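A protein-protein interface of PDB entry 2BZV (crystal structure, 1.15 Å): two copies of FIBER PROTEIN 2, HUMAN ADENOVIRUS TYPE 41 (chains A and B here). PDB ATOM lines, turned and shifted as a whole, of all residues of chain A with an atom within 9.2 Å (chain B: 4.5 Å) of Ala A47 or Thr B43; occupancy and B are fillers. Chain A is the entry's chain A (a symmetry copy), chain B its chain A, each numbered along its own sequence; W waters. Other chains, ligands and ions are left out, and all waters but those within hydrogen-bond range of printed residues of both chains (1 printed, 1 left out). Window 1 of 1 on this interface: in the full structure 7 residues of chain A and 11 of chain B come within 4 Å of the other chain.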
ATOM      1  N   THR A  43      35.303 -30.641   1.375  1.00  0.00           N
ATOM      2  CA  THR A  43      36.102 -29.661   2.119  1.00  0.00           C
ATOM      3  C   THR A  43      35.208 -29.002   3.164  1.00  0.00           C
ATOM      4  O   THR A  43      34.091 -28.560   2.887  1.00  0.00           O
ATOM      5  CB  THR A  43      36.789 -28.614   1.214  1.00  0.00           C
ATOM      6  OG1 THR A  43      35.808 -27.893   0.465  1.00  0.00           O
ATOM      7  CG2 THR A  43      37.746 -29.305   0.266  1.00  0.00           C
ATOM      8  N   LYS A  44      35.717 -28.965   4.396  1.00  0.00           N
ATOM      9  CA  LYS A  44      34.968 -28.466   5.544  1.00  0.00           C
ATOM     10  C   LYS A  44      35.338 -27.013   5.824  1.00  0.00           C
ATOM     11  O   LYS A  44      36.521 -26.678   5.955  1.00  0.00           O
ATOM     12  CB  LYS A  44      35.285 -29.318   6.776  1.00  0.00           C
ATOM     13  CG  LYS A  44      34.552 -28.850   8.022  1.00  0.00           C
ATOM     14  CD  LYS A  44      34.903 -29.708   9.228  1.00  0.00           C
ATOM     15  CE  LYS A  44      34.272 -29.185  10.506  1.00  0.00           C
ATOM     16  NZ  LYS A  44      32.790 -29.309  10.486  1.00  0.00           N
ATOM     17  N   ASN A  45      34.311 -26.166   5.924  1.00  0.00           N
ATOM     18  CA  ASN A  45      34.440 -24.750   6.295  1.00  0.00           C
ATOM     19  C   ASN A  45      33.459 -24.549   7.433  1.00  0.00           C
ATOM     20  O   ASN A  45      32.280 -24.307   7.173  1.00  0.00           O
ATOM     21  CB  ASN A  45      34.040 -23.872   5.068  1.00  0.00           C
ATOM     22  CG  ASN A  45      33.879 -22.360   5.296  1.00  0.00           C
ATOM     23  OD1 ASN A  45      34.717 -21.791   5.991  1.00  0.00           O
ATOM     24  ND2 ASN A  45      32.899 -21.685   4.657  1.00  0.00           N
ATOM     25  N   GLY A  46      33.902 -24.686   8.686  1.00  0.00           N
ATOM     26  CA  GLY A  46      32.974 -24.619   9.814  1.00  0.00           C
ATOM     27  C   GLY A  46      31.898 -25.677   9.672  1.00  0.00           C
ATOM     28  O   GLY A  46      32.198 -26.837   9.356  1.00  0.00           O
ATOM     29  N   ALA A  47      30.638 -25.281   9.839  1.00  0.00           N
ATOM     30  CA  ALA A  47      29.536 -26.226   9.796  1.00  0.00           C
ATOM     31  C   ALA A  47      29.149 -26.663   8.395  1.00  0.00           C
ATOM     32  O   ALA A  47      28.265 -27.511   8.269  1.00  0.00           O
ATOM     33  CB  ALA A  47      28.325 -25.651  10.514  1.00  0.00           C
ATOM     34  N   HIS A  48      29.760 -26.095   7.341  1.00  0.00           N
ATOM     35  CA  HIS A  48      29.457 -26.533   5.985  1.00  0.00           C
ATOM     36  C   HIS A  48      30.551 -27.420   5.424  1.00  0.00           C
ATOM     37  O   HIS A  48      31.743 -27.154   5.624  1.00  0.00           O
ATOM     38  CB  HIS A  48      29.360 -25.337   5.039  1.00  0.00           C
ATOM     39  CG  HIS A  48      28.006 -24.675   5.011  1.00  0.00           C
ATOM     40  ND1 HIS A  48      27.860 -23.309   4.984  1.00  0.00           N
ATOM     41  CD2 HIS A  48      26.751 -25.192   4.966  1.00  0.00           C
ATOM     42  CE1 HIS A  48      26.560 -23.013   4.928  1.00  0.00           C
ATOM     43  NE2 HIS A  48      25.865 -24.142   4.912  1.00  0.00           N
ATOM     44  N   VAL A  49      30.138 -28.420   4.655  1.00  0.00           N
ATOM     45  CA  VAL A  49      31.036 -29.076   3.716  1.00  0.00           C
ATOM     46  C   VAL A  49      30.566 -28.764   2.296  1.00  0.00           C
ATOM     47  O   VAL A  49      29.369 -28.781   1.999  1.00  0.00           O
ATOM     48  CB  VAL A  49      31.103 -30.595   3.939  1.00  0.00           C
ATOM     49  CG1 VAL A  49      31.608 -31.333   2.699  1.00  0.00           C
ATOM     50  CG2 VAL A  49      32.013 -30.894   5.117  1.00  0.00           C
ATOM     51  N   LEU A  50      31.539 -28.432   1.464  1.00  0.00           N
ATOM     52  CA  LEU A  50      31.377 -28.314   0.030  1.00  0.00           C
ATOM     53  C   LEU A  50      31.895 -29.605  -0.603  1.00  0.00           C
ATOM     54  O   LEU A  50      33.031 -30.001  -0.349  1.00  0.00           O
ATOM     55  CB  LEU A  50      32.207 -27.134  -0.460  1.00  0.00           C
ATOM     56  CG  LEU A  50      32.078 -26.702  -1.890  1.00  0.00           C
ATOM     57  CD1 LEU A  50      30.638 -26.313  -2.234  1.00  0.00           C
ATOM     58  CD2 LEU A  50      32.997 -25.494  -2.115  1.00  0.00           C
ATOM     59  N   THR A 106      33.357 -34.851  12.062  1.00  0.00           N
ATOM     60  CA  THR A 106      32.939 -33.478  11.746  1.00  0.00           C
ATOM     61  C   THR A 106      32.791 -33.228  10.250  1.00  0.00           C
ATOM     62  O   THR A 106      32.497 -32.099   9.853  1.00  0.00           O
ATOM     63  CB  THR A 106      33.863 -32.426  12.381  1.00  0.00           C
ATOM     64  OG1 THR A 106      35.170 -32.523  11.802  1.00  0.00           O
ATOM     65  CG2 THR A 106      33.941 -32.601  13.897  1.00  0.00           C
ATOM     66  N   PHE A 107      32.956 -34.270   9.431  1.00  0.00           N
ATOM     67  CA  PHE A 107      32.561 -34.235   8.024  1.00  0.00           C
ATOM     68  C   PHE A 107      31.241 -34.975   7.800  1.00  0.00           C
ATOM     69  O   PHE A 107      30.741 -35.003   6.671  1.00  0.00           O
ATOM     70  CB  PHE A 107      33.628 -34.892   7.138  1.00  0.00           C
ATOM     71  CG  PHE A 107      34.895 -34.094   6.980  1.00  0.00           C
ATOM     72  CD1 PHE A 107      35.174 -33.459   5.776  1.00  0.00           C
ATOM     73  CD2 PHE A 107      35.827 -33.997   8.009  1.00  0.00           C
ATOM     74  CE1 PHE A 107      36.346 -32.745   5.601  1.00  0.00           C
ATOM     75  CE2 PHE A 107      37.004 -33.279   7.838  1.00  0.00           C
ATOM     76  CZ  PHE A 107      37.257 -32.649   6.633  1.00  0.00           C
ATOM     77  N   MET A 108      30.673 -35.594   8.832  1.00  0.00           N
ATOM     78  CA  MET A 108      29.449 -36.364   8.641  1.00  0.00           C
ATOM     79  C   MET A 108      28.234 -35.450   8.548  1.00  0.00           C
ATOM     80  O   MET A 108      28.225 -34.385   9.162  1.00  0.00           O
ATOM     81  CB  MET A 108      29.254 -37.333   9.800  1.00  0.00           C
ATOM     82  CG  MET A 108      30.349 -38.392   9.871  1.00  0.00           C
ATOM     83  SD  MET A 108      30.419 -39.507   8.460  1.00  0.00           S
ATOM     84  CE  MET A 108      31.759 -38.801   7.465  1.00  0.00           C
ATOM     85  N   PRO A 109      27.211 -35.846   7.778  1.00  0.00           N
ATOM     86  CA  PRO A 109      25.997 -35.018   7.720  1.00  0.00           C
ATOM     87  C   PRO A 109      25.338 -34.957   9.101  1.00  0.00           C
ATOM     88  O   PRO A 109      25.116 -35.984   9.754  1.00  0.00           O
ATOM     89  CB  PRO A 109      25.123 -35.726   6.683  1.00  0.00           C
ATOM     90  CG  PRO A 109      26.022 -36.656   5.927  1.00  0.00           C
ATOM     91  CD  PRO A 109      27.118 -37.020   6.890  1.00  0.00           C
ATOM     92  N   ASN A 110      25.024 -33.735   9.532  1.00  0.00           N
ATOM     93  CA  ASN A 110      24.485 -33.479  10.852  1.00  0.00           C
ATOM     94  C   ASN A 110      23.224 -34.302  11.101  1.00  0.00           C
ATOM     95  O   ASN A 110      22.300 -34.280  10.280  1.00  0.00           O
ATOM     96  CB  ASN A 110      24.174 -31.988  10.935  1.00  0.00           C
ATOM     97  CG  ASN A 110      23.798 -31.526  12.316  1.00  0.00           C
ATOM     98  OD1 ASN A 110      22.710 -31.853  12.805  1.00  0.00           O
ATOM     99  ND2 ASN A 110      24.666 -30.766  12.965  1.00  0.00           N
ATOM    100  N   VAL A 113      20.004 -32.012  11.666  1.00  0.00           N
ATOM    101  CA  VAL A 113      19.509 -31.433  10.416  1.00  0.00           C
ATOM    102  C   VAL A 113      19.008 -32.528   9.463  1.00  0.00           C
ATOM    103  O   VAL A 113      17.999 -32.335   8.783  1.00  0.00           O
ATOM    104  CB  VAL A 113      20.605 -30.556   9.745  1.00  0.00           C
ATOM    105  CG1 VAL A 113      20.151 -30.015   8.391  1.00  0.00           C
ATOM    106  CG2 VAL A 113      21.000 -29.417  10.673  1.00  0.00           C
ATOM    107  N   TYR A 114      19.710 -33.672   9.434  1.00  0.00           N
ATOM    108  CA  TYR A 114      19.361 -34.806   8.581  1.00  0.00           C
ATOM    109  C   TYR A 114      19.209 -36.050   9.455  1.00  0.00           C
ATOM    110  O   TYR A 114      20.093 -36.898   9.534  1.00  0.00           O
ATOM    111  CB  TYR A 114      20.438 -35.048   7.506  1.00  0.00           C
ATOM    112  CG  TYR A 114      20.966 -33.793   6.844  1.00  0.00           C
ATOM    113  CD1 TYR A 114      20.249 -33.112   5.869  1.00  0.00           C
ATOM    114  CD2 TYR A 114      22.213 -33.302   7.195  1.00  0.00           C
ATOM    115  CE1 TYR A 114      20.762 -31.958   5.267  1.00  0.00           C
ATOM    116  CE2 TYR A 114      22.742 -32.165   6.606  1.00  0.00           C
ATOM    117  CZ  TYR A 114      22.014 -31.499   5.648  1.00  0.00           C
ATOM    118  OH  TYR A 114      22.566 -30.362   5.097  1.00  0.00           O
ATOM    119  N   CYS A 168      26.339 -29.161  -1.058  1.00  0.00           N
ATOM    120  CA  CYS A 168      26.729 -28.511   0.190  1.00  0.00           C
ATOM    121  C   CYS A 168      25.823 -29.045   1.308  1.00  0.00           C
ATOM    122  O   CYS A 168      24.599 -29.053   1.098  1.00  0.00           O
ATOM    123  CB  CYS A 168      26.580 -26.983   0.053  1.00  0.00           C
ATOM    124  SG  CYS A 168      26.883 -26.063   1.564  1.00  0.00           S
ATOM    125  N   TYR A 169      26.367 -29.398   2.464  1.00  0.00           N
ATOM    126  CA  TYR A 169      25.548 -29.864   3.576  1.00  0.00           C
ATOM    127  C   TYR A 169      26.136 -29.385   4.900  1.00  0.00           C
ATOM    128  O   TYR A 169      27.272 -28.903   4.973  1.00  0.00           O
ATOM    129  CB  TYR A 169      25.385 -31.398   3.532  1.00  0.00           C
ATOM    130  CG  TYR A 169      26.702 -32.131   3.728  1.00  0.00           C
ATOM    131  CD1 TYR A 169      27.121 -32.526   4.995  1.00  0.00           C
ATOM    132  CD2 TYR A 169      27.527 -32.421   2.640  1.00  0.00           C
ATOM    133  CE1 TYR A 169      28.337 -33.196   5.175  1.00  0.00           C
ATOM    134  CE2 TYR A 169      28.742 -33.081   2.808  1.00  0.00           C
ATOM    135  CZ  TYR A 169      29.141 -33.458   4.085  1.00  0.00           C
ATOM    136  OH  TYR A 169      30.359 -34.095   4.228  1.00  0.00           O
ATOM    137  N   ILE A 170      25.313 -29.503   5.946  1.00  0.00           N
ATOM    138  CA  ILE A 170      25.661 -29.141   7.306  1.00  0.00           C
ATOM    139  C   ILE A 170      26.254 -30.350   8.029  1.00  0.00           C
ATOM    140  O   ILE A 170      25.698 -31.456   7.946  1.00  0.00           O
ATOM    141  CB  ILE A 170      24.413 -28.682   8.075  1.00  0.00           C
ATOM    142  CG1 ILE A 170      23.651 -27.584   7.320  1.00  0.00           C
ATOM    143  CG2 ILE A 170      24.777 -28.264   9.500  1.00  0.00           C
ATOM    144  CD1 ILE A 170      24.377 -26.282   7.270  1.00  0.00           C
ATOM    145  N   THR A 171      27.363 -30.136   8.727  1.00  0.00           N
ATOM    146  CA  THR A 171      28.066 -31.237   9.367  1.00  0.00           C
ATOM    147  C   THR A 171      27.690 -31.422  10.823  1.00  0.00           C
ATOM    148  O   THR A 171      27.187 -30.517  11.494  1.00  0.00           O
ATOM    149  CB  THR A 171      29.602 -31.052   9.326  1.00  0.00           C
ATOM    150  OG1 THR A 171      29.989 -29.989  10.202  1.00  0.00           O
ATOM    151  CG2 THR A 171      30.077 -30.775   7.913  1.00  0.00           C
ATOM    152  N   GLU A 172      27.969 -32.617  11.302  1.00  0.00           N
ATOM    153  CA  GLU A 172      27.920 -32.956  12.704  1.00  0.00           C
ATOM    154  C   GLU A 172      28.993 -32.166  13.444  1.00  0.00           C
ATOM    155  O   GLU A 172      30.043 -31.854  12.868  1.00  0.00           O
ATOM    156  CB  GLU A 172      28.156 -34.475  12.812  1.00  0.00           C
ATOM    157  CG  GLU A 172      27.646 -35.215  13.995  1.00  0.00           C
ATOM    158  CD  GLU A 172      26.137 -35.273  14.142  1.00  0.00           C
ATOM    159  OE1 GLU A 172      25.426 -34.262  13.996  1.00  0.00           O
ATOM    160  OE2 GLU A 172      25.640 -36.367  14.429  1.00  0.00           O
ATOM    161  N   GLN A 173      28.712 -31.831  14.699  1.00  0.00           N
ATOM    162  CA  GLN A 173      29.740 -31.174  15.500  1.00  0.00           C
ATOM    163  C   GLN A 173      30.422 -32.201  16.380  1.00  0.00           C
ATOM    164  O   GLN A 173      29.903 -33.299  16.624  1.00  0.00           O
ATOM    165  CB  GLN A 173      29.182 -30.023  16.331  1.00  0.00           C
ATOM    166  CG  GLN A 173      28.967 -28.760  15.512  1.00  0.00           C
ATOM    167  CD  GLN A 173      28.119 -28.990  14.281  1.00  0.00           C
ATOM    168  OE1 GLN A 173      26.968 -29.403  14.415  1.00  0.00           O
ATOM    169  NE2 GLN A 173      28.680 -28.712  13.095  1.00  0.00           N
ATOM    170  N   THR B  17      33.994 -18.978  12.337  1.00  0.00           N
ATOM    171  CA  THR B  17      33.695 -19.352  10.956  1.00  0.00           C
ATOM    172  C   THR B  17      32.188 -19.386  10.652  1.00  0.00           C
ATOM    173  O   THR B  17      31.787 -19.196   9.508  1.00  0.00           O
ATOM    174  CB  THR B  17      34.314 -20.764  10.618  1.00  0.00           C
ATOM    175  OG1 THR B  17      33.576 -21.799  11.299  1.00  0.00           O
ATOM    176  CG2 THR B  17      35.840 -20.843  11.025  1.00  0.00           C
ATOM    177  N   THR B  18      31.379 -19.702  11.659  1.00  0.00           N
ATOM    178  CA  THR B  18      29.996 -20.098  11.418  1.00  0.00           C
ATOM    179  C   THR B  18      29.012 -19.307  12.269  1.00  0.00           C
ATOM    180  O   THR B  18      29.173 -19.216  13.490  1.00  0.00           O
ATOM    181  CB  THR B  18      29.807 -21.598  11.762  1.00  0.00           C
ATOM    182  OG1 THR B  18      30.728 -22.392  11.010  1.00  0.00           O
ATOM    183  CG2 THR B  18      28.405 -22.074  11.468  1.00  0.00           C
ATOM    184  N   TRP B  20      24.747 -19.515  12.852  1.00  0.00           N
ATOM    185  CA  TRP B  20      23.527 -20.205  12.442  1.00  0.00           C
ATOM    186  C   TRP B  20      22.374 -19.868  13.369  1.00  0.00           C
ATOM    187  O   TRP B  20      22.557 -19.298  14.438  1.00  0.00           O
ATOM    188  CB  TRP B  20      23.762 -21.713  12.276  1.00  0.00           C
ATOM    189  CG  TRP B  20      24.043 -22.515  13.513  1.00  0.00           C
ATOM    190  CD1 TRP B  20      24.061 -22.112  14.827  1.00  0.00           C
ATOM    191  CD2 TRP B  20      24.333 -23.919  13.526  1.00  0.00           C
ATOM    192  NE1 TRP B  20      24.345 -23.183  15.646  1.00  0.00           N
ATOM    193  CE2 TRP B  20      24.520 -24.300  14.864  1.00  0.00           C
ATOM    194  CE3 TRP B  20      24.465 -24.892  12.524  1.00  0.00           C
ATOM    195  CZ2 TRP B  20      24.814 -25.610  15.243  1.00  0.00           C
ATOM    196  CZ3 TRP B  20      24.760 -26.202  12.897  1.00  0.00           C
ATOM    197  CH2 TRP B  20      24.934 -26.543  14.245  1.00  0.00           C
ATOM    198  N   CYS B  41      22.334 -20.851   7.945  1.00  0.00           N
ATOM    199  CA  CYS B  41      23.696 -21.141   8.351  1.00  0.00           C
ATOM    200  C   CYS B  41      24.640 -20.429   7.390  1.00  0.00           C
ATOM    201  O   CYS B  41      24.526 -20.634   6.168  1.00  0.00           O
ATOM    202  CB  CYS B  41      23.944 -22.655   8.325  1.00  0.00           C
ATOM    203  SG  CYS B  41      25.625 -23.111   8.835  1.00  0.00           S
ATOM    204  N   LEU B  42      25.525 -19.596   7.932  1.00  0.00           N
ATOM    205  CA  LEU B  42      26.523 -18.842   7.171  1.00  0.00           C
ATOM    206  C   LEU B  42      27.899 -19.313   7.579  1.00  0.00           C
ATOM    207  O   LEU B  42      28.212 -19.296   8.769  1.00  0.00           O
ATOM    208  CB  LEU B  42      26.414 -17.340   7.490  1.00  0.00           C
ATOM    209  CG  LEU B  42      25.046 -16.685   7.267  1.00  0.00           C
ATOM    210  CD1 LEU B  42      25.111 -15.213   7.658  1.00  0.00           C
ATOM    211  CD2 LEU B  42      24.577 -16.853   5.831  1.00  0.00           C
ATOM    212  N   THR B  43      28.735 -19.665   6.603  1.00  0.00           N
ATOM    213  CA  THR B  43      30.130 -19.992   6.918  1.00  0.00           C
ATOM    214  C   THR B  43      31.037 -19.116   6.058  1.00  0.00           C
ATOM    215  O   THR B  43      30.864 -18.985   4.846  1.00  0.00           O
ATOM    216  CB  THR B  43      30.462 -21.492   6.752  1.00  0.00           C
ATOM    217  OG1 THR B  43      30.214 -21.904   5.406  1.00  0.00           O
ATOM    218  CG2 THR B  43      29.614 -22.312   7.700  1.00  0.00           C
ATOM    219  N   LYS B  44      32.008 -18.491   6.725  1.00  0.00           N
ATOM    220  CA  LYS B  44      32.909 -17.533   6.091  1.00  0.00           C
ATOM    221  C   LYS B  44      34.218 -18.216   5.707  1.00  0.00           C
ATOM    222  O   LYS B  44      34.860 -18.862   6.542  1.00  0.00           O
ATOM    223  CB  LYS B  44      33.200 -16.382   7.057  1.00  0.00           C
ATOM    224  CG  LYS B  44      34.147 -15.347   6.475  1.00  0.00           C
ATOM    225  CD  LYS B  44      34.427 -14.229   7.467  1.00  0.00           C
ATOM    226  CE  LYS B  44      35.462 -13.247   6.946  1.00  0.00           C
ATOM    227  NZ  LYS B  44      34.960 -12.477   5.778  1.00  0.00           N
ATOM    228  N   ASN B  45      34.601 -18.052   4.439  1.00  0.00           N
ATOM    229  CA  ASN B  45      35.879 -18.532   3.893  1.00  0.00           C
ATOM    230  C   ASN B  45      36.500 -17.325   3.219  1.00  0.00           C
ATOM    231  O   ASN B  45      36.180 -17.054   2.062  1.00  0.00           O
ATOM    232  CB  ASN B  45      35.586 -19.652   2.846  1.00  0.00           C
ATOM    233  CG  ASN B  45      36.759 -20.141   1.979  1.00  0.00           C
ATOM    234  OD1 ASN B  45      37.842 -20.323   2.528  1.00  0.00           O
ATOM    235  ND2 ASN B  45      36.551 -20.452   0.681  1.00  0.00           N
ATOM    236  N   HIS B  48      34.346 -14.832   0.933  1.00  0.00           N
ATOM    237  CA  HIS B  48      33.066 -15.455   0.618  1.00  0.00           C
ATOM    238  C   HIS B  48      32.371 -15.966   1.864  1.00  0.00           C
ATOM    239  O   HIS B  48      33.012 -16.533   2.757  1.00  0.00           O
ATOM    240  CB  HIS B  48      33.264 -16.673  -0.282  1.00  0.00           C
ATOM    241  CG  HIS B  48      33.346 -16.352  -1.753  1.00  0.00           C
ATOM    242  ND1 HIS B  48      34.253 -16.962  -2.586  1.00  0.00           N
ATOM    243  CD2 HIS B  48      32.612 -15.520  -2.536  1.00  0.00           C
ATOM    244  CE1 HIS B  48      34.073 -16.510  -3.829  1.00  0.00           C
ATOM    245  NE2 HIS B  48      33.077 -15.635  -3.825  1.00  0.00           N
ATOM    246  N   VAL B  49      31.049 -15.837   1.874  1.00  0.00           N
ATOM    247  CA  VAL B  49      30.215 -16.639   2.756  1.00  0.00           C
ATOM    248  C   VAL B  49      29.378 -17.590   1.902  1.00  0.00           C
ATOM    249  O   VAL B  49      28.847 -17.211   0.856  1.00  0.00           O
ATOM    250  CB  VAL B  49      29.308 -15.774   3.646  1.00  0.00           C
ATOM    251  CG1 VAL B  49      28.112 -16.562   4.180  1.00  0.00           C
ATOM    252  CG2 VAL B  49      30.115 -15.220   4.806  1.00  0.00           C
ATOM    253  N   LEU B  50      29.331 -18.829   2.360  1.00  0.00           N
ATOM    254  CA  LEU B  50      28.432 -19.848   1.858  1.00  0.00           C
ATOM    255  C   LEU B  50      27.247 -19.934   2.820  1.00  0.00           C
ATOM    256  O   LEU B  50      27.441 -20.114   4.021  1.00  0.00           O
ATOM    257  CB  LEU B  50      29.168 -21.181   1.831  1.00  0.00           C
ATOM    258  CG  LEU B  50      28.501 -22.365   1.195  1.00  0.00           C
ATOM    259  CD1 LEU B  50      28.160 -22.098  -0.273  1.00  0.00           C
ATOM    260  CD2 LEU B  50      29.456 -23.562   1.285  1.00  0.00           C
ATOM    261  N   GLN B  95      28.171 -20.661  15.984  1.00  0.00           N
ATOM    262  CA  GLN B  95      28.077 -22.076  16.286  1.00  0.00           C
ATOM    263  C   GLN B  95      29.217 -22.549  17.184  1.00  0.00           C
ATOM    264  O   GLN B  95      29.010 -23.390  18.056  1.00  0.00           O
ATOM    265  CB  GLN B  95      28.011 -22.854  14.971  1.00  0.00           C
ATOM    266  CG  GLN B  95      28.033 -24.341  15.160  1.00  0.00           C
ATOM    267  CD  GLN B  95      29.425 -24.848  14.942  1.00  0.00           C
ATOM    268  OE1 GLN B  95      30.092 -24.470  13.987  1.00  0.00           O
ATOM    269  NE2 GLN B  95      29.877 -25.672  15.862  1.00  0.00           N
HETATM  270  O   HOH W   1      32.694 -19.827   2.336  1.00  0.00           O
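The backbone NH (N) of Ala A47 is in hydrogen-bond range of the side-chain hydroxyl (OG1) of Thr B18 (3.1 Å).
The side-chain hydroxyl of Thr B43 lies within hydrogen-bond range of the side-chain amide nitrogen of Asn A45 (2.8 Å).
The side-chain hydroxyl of Thr B43 is in hydrogen-bond range of a ring nitrogen (ND1) of His A48 (2.8 Å).
The backbone carbonyl oxygen of Lys B44 sits close to the side-chain amide oxygen of Asn A45, 3.0 Å away.
The backbone carbonyl oxygen (O) of Leu B50 lies close to a ring nitrogen (ND1) of His A48, at 3.4 Å.
The side-chain hydroxyl (OG1) of Thr B17 sits at hydrogen-bond distance from the side-chain hydroxyl (OG1) of Thr B18 (2.9 Å).
O of Thr B17 sits at hydrogen-bond distance from N of Lys B44.
O of Gly A46 is in hydrogen-bond range of NZ of Lys A44 (2.8 Å).
The backbone carbonyl oxygen (O) of Ala A47 lies within hydrogen-bond range of the backbone NH (N) of Thr A171, 2.8 Å away.
The backbone carbonyl oxygen (O) of Ile A170 sits at hydrogen-bond distance from the backbone NH (N) of Asn A110, at 2.9 Å.
The side-chain amide nitrogen (ND2) of Asn A110 sits at hydrogen-bond distance from the side-chain amide oxygen (OE1) of Gln A173, at 3.0 Å.
Among the printed residues, merely in contact across the chains: Asn A45 with Asn B45, Gly A46 with Thr B17, Gly A46 with Thr B18, Ala A47 with Thr B43, His A48 with Cys B41, Cys A168 with Leu B50, Ile A170 with Trp B20, Ile A170 with Cys B41, Gln A173 with Trp B20 and Gln A173 with Gln B95.
Of chain A, only Asn A45 (2.8 Å), Ala A47 (3.8 Å) and His A48 (2.8 Å) come within 4 Å of Thr B43.
No residue of chain A comes within 4 Å of Val B49.
Of the printed residues of chain B, Gly A46 touches Thr B17 and Thr B18.
Printed residues of chain B within 4 Å of Gln A173: Trp B20 (3.5 Å) and Gln B95 (3.2 Å).
Printed residues of chain A within 4 Å of Lys B44: Asn A45.
Of the printed residues of chain B, His A48 touches Cys B41, Thr B43 and Leu B50.
Printed residues of chain A within 4 Å of Leu B50: His A48 (3.2 Å) and Cys A168 (3.6 Å).
Asn A110 touches none of the printed residues of chain B.
Glu A172 touches none of the printed residues of chain B.
The nearest printed residue of chain B that does not touch Ala A47 is Cys B41 (4.1 Å).
The nearest residue of chain A that does not touch Thr B43 is Gly A46 (4.5 Å).
Along chain A the printed residues that touch a printed residue of chain B span positions 45 to 173.
Hydrophobic or aromatic side chains of chain B within 4 Å of the printed part of chain A: Trp B20 and Leu B50.
Asn A45 touches Lys B44, but with the chains exchanged Lys A44 does not touch Asn B45 (7.3 Å).
Asn A45 touches its own counterpart, Asn B45.
His A48 touches Thr B43, but with the chains exchanged Thr A43 does not touch His B48 (11.5 Å).
His A48 touches Leu B50, but with the chains exchanged Leu A50 does not touch His B48 (8.6 Å).
Of the 15 pairs that touch across the chains among the printed residues, 1 has its exchanged pair printed and touching as well.
Water W1 lies within hydrogen-bond range of the side-chain amide nitrogen (ND2) of Asn A45, the backbone carbonyl oxygen (O) of Thr B43, the backbone carbonyl oxygen (O) of His B48 and the backbone NH (N) of Asn B45.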
